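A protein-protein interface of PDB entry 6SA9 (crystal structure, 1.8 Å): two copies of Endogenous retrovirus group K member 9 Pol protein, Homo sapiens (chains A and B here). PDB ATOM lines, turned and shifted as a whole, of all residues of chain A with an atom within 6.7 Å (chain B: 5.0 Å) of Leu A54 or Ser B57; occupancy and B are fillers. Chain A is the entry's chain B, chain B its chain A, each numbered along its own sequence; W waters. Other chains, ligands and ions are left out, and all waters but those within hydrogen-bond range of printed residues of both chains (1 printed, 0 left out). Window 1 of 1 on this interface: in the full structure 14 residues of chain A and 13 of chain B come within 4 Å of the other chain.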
ATOM      1  N   LYS A  32      17.956  17.655 -19.082  1.00  0.00           N
ATOM      2  CA  LYS A  32      18.107  17.091 -20.426  1.00  0.00           C
ATOM      3  C   LYS A  32      18.972  15.827 -20.429  1.00  0.00           C
ATOM      4  O   LYS A  32      18.663  14.863 -21.123  1.00  0.00           O
ATOM      5  CB  LYS A  32      18.680  18.126 -21.398  1.00  0.00           C
ATOM      6  CG  LYS A  32      18.730  17.674 -22.858  1.00  0.00           C
ATOM      7  CD  LYS A  32      17.336  17.610 -23.487  1.00  0.00           C
ATOM      8  CE  LYS A  32      17.363  16.918 -24.846  1.00  0.00           C
ATOM      9  NZ  LYS A  32      18.270  17.613 -25.788  1.00  0.00           N
ATOM     10  N   MET A  33      20.059  15.841 -19.663  1.00  0.00           N
ATOM     11  CA  MET A  33      20.900  14.650 -19.519  1.00  0.00           C
ATOM     12  C   MET A  33      20.067  13.483 -18.975  1.00  0.00           C
ATOM     13  O   MET A  33      20.119  12.379 -19.512  1.00  0.00           O
ATOM     14  CB  MET A  33      22.079  14.937 -18.592  1.00  0.00           C
ATOM     15  CG  MET A  33      23.337  14.089 -18.819  1.00  0.00           C
ATOM     16  SD  MET A  33      23.839  13.367 -17.105  1.00  0.00           S
ATOM     17  CE  MET A  33      22.456  12.066 -17.392  1.00  0.00           C
ATOM     18  N   LYS A  35      16.862  13.041 -19.149  1.00  0.00           N
ATOM     19  CA  LYS A  35      15.917  12.645 -20.185  1.00  0.00           C
ATOM     20  C   LYS A  35      16.627  11.797 -21.241  1.00  0.00           C
ATOM     21  O   LYS A  35      16.116  10.758 -21.659  1.00  0.00           O
ATOM     22  CB  LYS A  35      15.278  13.883 -20.821  1.00  0.00           C
ATOM     23  CG  LYS A  35      14.190  13.599 -21.854  1.00  0.00           C
ATOM     24  CD  LYS A  35      13.727  14.900 -22.509  1.00  0.00           C
ATOM     25  CE  LYS A  35      12.290  14.820 -23.013  1.00  0.00           C
ATOM     26  NZ  LYS A  35      12.126  13.901 -24.174  1.00  0.00           N
ATOM     27  N   ASP A  36      17.816  12.237 -21.647  1.00  0.00           N
ATOM     28  CA  ASP A  36      18.635  11.505 -22.617  1.00  0.00           C
ATOM     29  C   ASP A  36      18.927  10.091 -22.127  1.00  0.00           C
ATOM     30  O   ASP A  36      18.859   9.118 -22.875  1.00  0.00           O
ATOM     31  CB  ASP A  36      19.976  12.223 -22.835  1.00  0.00           C
ATOM     32  CG  ASP A  36      19.860  13.449 -23.741  1.00  0.00           C
ATOM     33  OD1 ASP A  36      20.812  14.265 -23.764  1.00  0.00           O
ATOM     34  OD2 ASP A  36      18.825  13.603 -24.421  1.00  0.00           O
ATOM     35  N   MET A  37      19.264   9.983 -20.855  1.00  0.00           N
ATOM     36  CA  MET A  37      19.658   8.700 -20.310  1.00  0.00           C
ATOM     37  C   MET A  37      18.492   7.741 -20.168  1.00  0.00           C
ATOM     38  O   MET A  37      18.639   6.554 -20.431  1.00  0.00           O
ATOM     39  CB  MET A  37      20.364   8.886 -18.982  1.00  0.00           C
ATOM     40  CG  MET A  37      21.721   9.505 -19.146  1.00  0.00           C
ATOM     41  SD  MET A  37      22.842   8.838 -17.735  1.00  0.00           S
ATOM     42  CE  MET A  37      21.483   8.866 -16.357  1.00  0.00           C
ATOM     43  N   GLY A  40      17.800   6.552 -23.601  1.00  0.00           N
ATOM     44  CA  GLY A  40      18.872   5.667 -24.030  1.00  0.00           C
ATOM     45  C   GLY A  40      18.807   4.277 -23.417  1.00  0.00           C
ATOM     46  O   GLY A  40      19.033   3.277 -24.099  1.00  0.00           O
ATOM     47  N   PRO A  49      26.765  -0.973 -24.963  1.00  0.00           N
ATOM     48  CA  PRO A  49      27.963  -0.133 -25.066  1.00  0.00           C
ATOM     49  C   PRO A  49      27.588   1.350 -24.975  1.00  0.00           C
ATOM     50  O   PRO A  49      28.337   2.148 -24.416  1.00  0.00           O
ATOM     51  CB  PRO A  49      28.501  -0.478 -26.454  1.00  0.00           C
ATOM     52  CG  PRO A  49      28.070  -1.887 -26.664  1.00  0.00           C
ATOM     53  CD  PRO A  49      26.711  -1.994 -26.024  1.00  0.00           C
ATOM     54  N   TYR A  50      26.419   1.691 -25.512  1.00  0.00           N
ATOM     55  CA  TYR A  50      25.877   3.044 -25.428  1.00  0.00           C
ATOM     56  C   TYR A  50      25.852   3.541 -23.988  1.00  0.00           C
ATOM     57  O   TYR A  50      26.457   4.566 -23.656  1.00  0.00           O
ATOM     58  CB  TYR A  50      24.457   3.068 -26.000  1.00  0.00           C
ATOM     59  CG  TYR A  50      23.795   4.440 -26.056  1.00  0.00           C
ATOM     60  CD1 TYR A  50      23.258   5.029 -24.911  1.00  0.00           C
ATOM     61  CD2 TYR A  50      23.690   5.134 -27.253  1.00  0.00           C
ATOM     62  CE1 TYR A  50      22.641   6.277 -24.966  1.00  0.00           C
ATOM     63  CE2 TYR A  50      23.071   6.379 -27.318  1.00  0.00           C
ATOM     64  CZ  TYR A  50      22.554   6.950 -26.168  1.00  0.00           C
ATOM     65  OH  TYR A  50      21.936   8.187 -26.236  1.00  0.00           O
ATOM     66  N   MET A  51      25.147   2.814 -23.126  1.00  0.00           N
ATOM     67  CA  MET A  51      24.968   3.239 -21.738  1.00  0.00           C
ATOM     68  C   MET A  51      26.257   3.137 -20.932  1.00  0.00           C
ATOM     69  O   MET A  51      26.506   3.944 -20.046  1.00  0.00           O
ATOM     70  CB  MET A  51      23.861   2.432 -21.058  1.00  0.00           C
ATOM     71  CG  MET A  51      23.449   2.978 -19.701  1.00  0.00           C
ATOM     72  SD  MET A  51      23.102   4.905 -19.741  1.00  0.00           S
ATOM     73  CE  MET A  51      21.844   4.966 -21.235  1.00  0.00           C
ATOM     74  N   ARG A  52      27.077   2.136 -21.241  1.00  0.00           N
ATOM     75  CA  ARG A  52      28.331   1.973 -20.515  1.00  0.00           C
ATOM     76  C   ARG A  52      29.246   3.167 -20.761  1.00  0.00           C
ATOM     77  O   ARG A  52      29.862   3.684 -19.831  1.00  0.00           O
ATOM     78  CB  ARG A  52      29.033   0.678 -20.914  1.00  0.00           C
ATOM     79  CG  ARG A  52      28.417  -0.571 -20.315  1.00  0.00           C
ATOM     80  CD  ARG A  52      29.062  -1.822 -20.894  1.00  0.00           C
ATOM     81  NE  ARG A  52      28.699  -3.024 -20.149  1.00  0.00           N
ATOM     82  CZ  ARG A  52      29.291  -3.410 -19.023  1.00  0.00           C
ATOM     83  NH1 ARG A  52      30.274  -2.686 -18.504  1.00  0.00           N
ATOM     84  NH2 ARG A  52      28.897  -4.521 -18.412  1.00  0.00           N
ATOM     85  N   THR A  53      29.322   3.601 -22.014  1.00  0.00           N
ATOM     86  CA  THR A  53      30.127   4.761 -22.374  1.00  0.00           C
ATOM     87  C   THR A  53      29.663   5.994 -21.594  1.00  0.00           C
ATOM     88  O   THR A  53      30.453   6.655 -20.923  1.00  0.00           O
ATOM     89  CB  THR A  53      30.033   5.066 -23.875  1.00  0.00           C
ATOM     90  OG1 THR A  53      30.428   3.910 -24.635  1.00  0.00           O
ATOM     91  CG2 THR A  53      30.929   6.252 -24.227  1.00  0.00           C
ATOM     92  N   LEU A  54      28.368   6.277 -21.669  1.00  0.00           N
ATOM     93  CA  LEU A  54      27.796   7.443 -21.014  1.00  0.00           C
ATOM     94  C   LEU A  54      27.959   7.390 -19.494  1.00  0.00           C
ATOM     95  O   LEU A  54      28.432   8.336 -18.870  1.00  0.00           O
ATOM     96  CB  LEU A  54      26.316   7.583 -21.391  1.00  0.00           C
ATOM     97  CG  LEU A  54      25.529   8.733 -20.757  1.00  0.00           C
ATOM     98  CD1 LEU A  54      26.200  10.065 -21.024  1.00  0.00           C
ATOM     99  CD2 LEU A  54      24.101   8.744 -21.287  1.00  0.00           C
ATOM    100  N   LEU A  55      27.561   6.275 -18.894  1.00  0.00           N
ATOM    101  CA  LEU A  55      27.571   6.171 -17.437  1.00  0.00           C
ATOM    102  C   LEU A  55      28.985   6.236 -16.857  1.00  0.00           C
ATOM    103  O   LEU A  55      29.229   6.950 -15.883  1.00  0.00           O
ATOM    104  CB  LEU A  55      26.882   4.881 -17.001  1.00  0.00           C
ATOM    105  CG  LEU A  55      26.652   4.751 -15.505  1.00  0.00           C
ATOM    106  CD1 LEU A  55      25.689   5.841 -15.021  1.00  0.00           C
ATOM    107  CD2 LEU A  55      26.122   3.367 -15.206  1.00  0.00           C
ATOM    108  N   ASP A  56      29.913   5.491 -17.456  1.00  0.00           N
ATOM    109  CA  ASP A  56      31.308   5.512 -17.006  1.00  0.00           C
ATOM    110  C   ASP A  56      31.865   6.933 -17.035  1.00  0.00           C
ATOM    111  O   ASP A  56      32.558   7.363 -16.107  1.00  0.00           O
ATOM    112  CB  ASP A  56      32.182   4.582 -17.866  1.00  0.00           C
ATOM    113  CG  ASP A  56      31.897   3.107 -17.614  1.00  0.00           C
ATOM    114  OD1 ASP A  56      32.455   2.254 -18.342  1.00  0.00           O
ATOM    115  OD2 ASP A  56      31.113   2.799 -16.689  1.00  0.00           O
ATOM    116  N   SER A  57      31.550   7.673 -18.090  1.00  0.00           N
ATOM    117  CA  SER A  57      32.062   9.036 -18.208  1.00  0.00           C
ATOM    118  C   SER A  57      31.496   9.945 -17.117  1.00  0.00           C
ATOM    119  O   SER A  57      32.204  10.793 -16.577  1.00  0.00           O
ATOM    120  CB  SER A  57      31.783   9.623 -19.598  1.00  0.00           C
ATOM    121  OG  SER A  57      30.479  10.175 -19.680  1.00  0.00           O
ATOM    122  N   ILE A  58      30.217   9.774 -16.797  1.00  0.00           N
ATOM    123  CA  ILE A  58      29.591  10.590 -15.758  1.00  0.00           C
ATOM    124  C   ILE A  58      30.164  10.238 -14.389  1.00  0.00           C
ATOM    125  O   ILE A  58      30.493  11.124 -13.601  1.00  0.00           O
ATOM    126  CB  ILE A  58      28.059  10.426 -15.752  1.00  0.00           C
ATOM    127  CG1 ILE A  58      27.467  10.964 -17.054  1.00  0.00           C
ATOM    128  CG2 ILE A  58      27.440  11.174 -14.576  1.00  0.00           C
ATOM    129  CD1 ILE A  58      25.989  10.811 -17.123  1.00  0.00           C
ATOM    130  N   ALA A  59      30.305   8.941 -14.127  1.00  0.00           N
ATOM    131  CA  ALA A  59      30.774   8.463 -12.831  1.00  0.00           C
ATOM    132  C   ALA A  59      32.203   8.890 -12.522  1.00  0.00           C
ATOM    133  O   ALA A  59      32.529   9.190 -11.370  1.00  0.00           O
ATOM    134  CB  ALA A  59      30.653   6.950 -12.749  1.00  0.00           C
ATOM    135  N   THR B  53      22.280  11.086 -29.961  1.00  0.00           N
ATOM    136  CA  THR B  53      21.772  11.151 -28.602  1.00  0.00           C
ATOM    137  C   THR B  53      22.904  10.919 -27.585  1.00  0.00           C
ATOM    138  O   THR B  53      22.914  11.520 -26.509  1.00  0.00           O
ATOM    139  CB  THR B  53      20.557  10.218 -28.405  1.00  0.00           C
ATOM    140  OG1 THR B  53      20.950   8.858 -28.579  1.00  0.00           O
ATOM    141  CG2 THR B  53      19.471  10.553 -29.431  1.00  0.00           C
ATOM    142  N   LEU B  54      23.884  10.093 -27.938  1.00  0.00           N
ATOM    143  CA  LEU B  54      25.028   9.871 -27.054  1.00  0.00           C
ATOM    144  C   LEU B  54      25.814  11.170 -26.893  1.00  0.00           C
ATOM    145  O   LEU B  54      26.178  11.562 -25.782  1.00  0.00           O
ATOM    146  CB  LEU B  54      25.937   8.770 -27.599  1.00  0.00           C
ATOM    147  CG  LEU B  54      27.164   8.401 -26.762  1.00  0.00           C
ATOM    148  CD1 LEU B  54      26.753   7.962 -25.356  1.00  0.00           C
ATOM    149  CD2 LEU B  54      27.961   7.308 -27.444  1.00  0.00           C
ATOM    150  N   LEU B  55      26.059  11.849 -28.011  1.00  0.00           N
ATOM    151  CA  LEU B  55      26.740  13.132 -27.973  1.00  0.00           C
ATOM    152  C   LEU B  55      25.949  14.169 -27.175  1.00  0.00           C
ATOM    153  O   LEU B  55      26.516  14.923 -26.378  1.00  0.00           O
ATOM    154  CB  LEU B  55      26.982  13.631 -29.391  1.00  0.00           C
ATOM    155  CG  LEU B  55      27.920  14.826 -29.508  1.00  0.00           C
ATOM    156  CD1 LEU B  55      29.296  14.482 -28.952  1.00  0.00           C
ATOM    157  CD2 LEU B  55      28.001  15.254 -30.971  1.00  0.00           C
ATOM    158  N   ASP B  56      24.637  14.200 -27.389  1.00  0.00           N
ATOM    159  CA  ASP B  56      23.774  15.107 -26.645  1.00  0.00           C
ATOM    160  C   ASP B  56      23.880  14.855 -25.145  1.00  0.00           C
ATOM    161  O   ASP B  56      23.959  15.801 -24.352  1.00  0.00           O
ATOM    162  CB  ASP B  56      22.317  14.963 -27.085  1.00  0.00           C
ATOM    163  CG  ASP B  56      21.458  16.144 -26.632  1.00  0.00           C
ATOM    164  OD1 ASP B  56      20.846  16.069 -25.547  1.00  0.00           O
ATOM    165  OD2 ASP B  56      21.427  17.164 -27.350  1.00  0.00           O
ATOM    166  N   SER B  57      23.883  13.577 -24.765  1.00  0.00           N
ATOM    167  CA  SER B  57      23.970  13.171 -23.362  1.00  0.00           C
ATOM    168  C   SER B  57      25.279  13.614 -22.731  1.00  0.00           C
ATOM    169  O   SER B  57      25.299  14.159 -21.627  1.00  0.00           O
ATOM    170  CB  SER B  57      23.826  11.651 -23.227  1.00  0.00           C
ATOM    171  OG  SER B  57      22.598  11.198 -23.778  1.00  0.00           O
ATOM    172  N   ILE B  58      26.379  13.355 -23.433  1.00  0.00           N
ATOM    173  CA  ILE B  58      27.703  13.765 -22.969  1.00  0.00           C
ATOM    174  C   ILE B  58      27.791  15.283 -22.838  1.00  0.00           C
ATOM    175  O   ILE B  58      28.343  15.803 -21.854  1.00  0.00           O
ATOM    176  CB  ILE B  58      28.800  13.248 -23.930  1.00  0.00           C
ATOM    177  CG1 ILE B  58      28.959  11.737 -23.781  1.00  0.00           C
ATOM    178  CG2 ILE B  58      30.126  13.953 -23.674  1.00  0.00           C
ATOM    179  CD1 ILE B  58      29.655  11.091 -24.944  1.00  0.00           C
ATOM    180  N   ALA B  59      27.231  15.987 -23.821  1.00  0.00           N
ATOM    181  CA  ALA B  59      27.274  17.451 -23.862  1.00  0.00           C
ATOM    182  C   ALA B  59      26.449  18.111 -22.747  1.00  0.00           C
ATOM    183  O   ALA B  59      26.735  19.244 -22.343  1.00  0.00           O
ATOM    184  CB  ALA B  59      26.832  17.961 -25.244  1.00  0.00           C
ATOM    185  N   HIS B  60      25.427  17.414 -22.255  1.00  0.00           N
ATOM    186  CA  HIS B  60      24.613  17.929 -21.154  1.00  0.00           C
ATOM    187  C   HIS B  60      25.050  17.350 -19.813  1.00  0.00           C
ATOM    188  O   HIS B  60      24.705  17.882 -18.757  1.00  0.00           O
ATOM    189  CB  HIS B  60      23.127  17.645 -21.388  1.00  0.00           C
ATOM    190  CG  HIS B  60      22.501  18.538 -22.414  1.00  0.00           C
ATOM    191  ND1 HIS B  60      22.567  18.277 -23.766  1.00  0.00           N
ATOM    192  CD2 HIS B  60      21.809  19.695 -22.288  1.00  0.00           C
ATOM    193  CE1 HIS B  60      21.940  19.233 -24.429  1.00  0.00           C
ATOM    194  NE2 HIS B  60      21.471  20.106 -23.555  1.00  0.00           N
ATOM    195  N   GLY B  61      25.814  16.263 -19.867  1.00  0.00           N
ATOM    196  CA  GLY B  61      26.282  15.583 -18.674  1.00  0.00           C
ATOM    197  C   GLY B  61      27.587  16.139 -18.137  1.00  0.00           C
ATOM    198  O   GLY B  61      27.930  15.922 -16.974  1.00  0.00           O
ATOM    199  N   HIS B  62      28.308  16.849 -19.001  1.00  0.00           N
ATOM    200  CA  HIS B  62      29.598  17.427 -18.668  1.00  0.00           C
ATOM    201  C   HIS B  62      29.608  18.878 -19.108  1.00  0.00           C
ATOM    202  O   HIS B  62      28.838  19.284 -19.982  1.00  0.00           O
ATOM    203  CB  HIS B  62      30.714  16.701 -19.420  1.00  0.00           C
ATOM    204  CG  HIS B  62      30.828  15.246 -19.088  1.00  0.00           C
ATOM    205  ND1 HIS B  62      31.447  14.793 -17.945  1.00  0.00           N
ATOM    206  CD2 HIS B  62      30.425  14.142 -19.762  1.00  0.00           C
ATOM    207  CE1 HIS B  62      31.419  13.472 -17.924  1.00  0.00           C
ATOM    208  NE2 HIS B  62      30.805  13.053 -19.016  1.00  0.00           N
HETATM  209  O   HOH W   1      20.381  19.514 -26.743  1.00  0.00           O
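The side-chain carboxylate of Asp A36 sits at hydrogen-bond distance from the backbone NH of Ser B57 (3.3 Å).
The side-chain hydroxyl of Tyr A50 is in hydrogen-bond range of the backbone NH of Leu B54, 3.2 Å away.
OD1 of Asp B56 lies within salt-bridge range of NZ of Lys A32, at 3.0 Å.
The side-chain hydroxyl (OG1) of Thr B53 lies within hydrogen-bond range of the side-chain hydroxyl (OH) of Tyr A50, at 2.6 Å.
NE2 of His B62 lies within hydrogen-bond range of OG of Ser A57 (3.0 Å).
The side-chain carboxylate (OD1) of Asp B56 sits close to the side-chain carboxylate (OD1) of Asp A36, 2.5 Å away.
O of Leu A54 lies within hydrogen-bond range of OG of Ser A57, 2.9 Å away.
OG of Ser B57 sits at hydrogen-bond distance from O of Thr B53 (2.8 Å).
ND1 of His B60 is in hydrogen-bond range of O of Asp B56.
Among the printed residues, pairs that only touch across the chains: Met A33 with Gly B61 (3.3 Å), Met A33 with Ser B57 (3.4 Å), Leu A54 with Ser B57 (3.5 Å), Lys A32 with His B60 (3.6 Å), Met A33 with His B60 (3.8 Å) and Tyr A50 with Ser B57 (3.9 Å).
Ser B57 touches four residues of chain A.
Printed residues of chain B within 4 Å of Lys A32: Asp B56 (3.0 Å) and His B60 (3.6 Å).
Of the printed residues of chain A, Thr B53 touches Tyr A50.
Of the printed residues of chain A, His B60 touches Lys A32 and Met A33.
The nearest printed residue of chain B that does not touch Leu A54 is Leu B54 (4.01 Å).
The nearest printed residue of chain A that does not touch Ser B57 is Met A37 (4.6 Å).
The nearest printed residue of chain B that does not touch Asp A36 is His B60 (4.4 Å).
Hydrophobic or aromatic side chains of chain B that line the printed part of chain A: Leu B54, His B60 and His B62.
Of the 17 printed residues of chain A, 6 touch a printed residue of chain B.
Printed residues of chain A that touch a printed residue of chain B: Lys A32, Met A33, Asp A36, Tyr A50, Leu A54 and Ser A57.
Among the printed residues, Asp or Glu carboxylates within 4 Å of a Lys or Arg side-chain nitrogen of the other chain: Lys A32 with Asp B56.
Leu A54 touches Ser B57, but with the chains exchanged Ser A57 does not touch Leu B54 (7.1 Å).
Of the 12 pairs that touch across the chains among the printed residues, none has its exchanged pair printed and touching as well.
Water W1 lies within hydrogen-bond range of the side-chain carboxylate (OD2) of Asp B56 (2.6 Å), the side-chain amino group (NZ) of Lys A32 (3.0 Å) and a ring nitrogen (NE2) of His B60 (3.4 Å).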
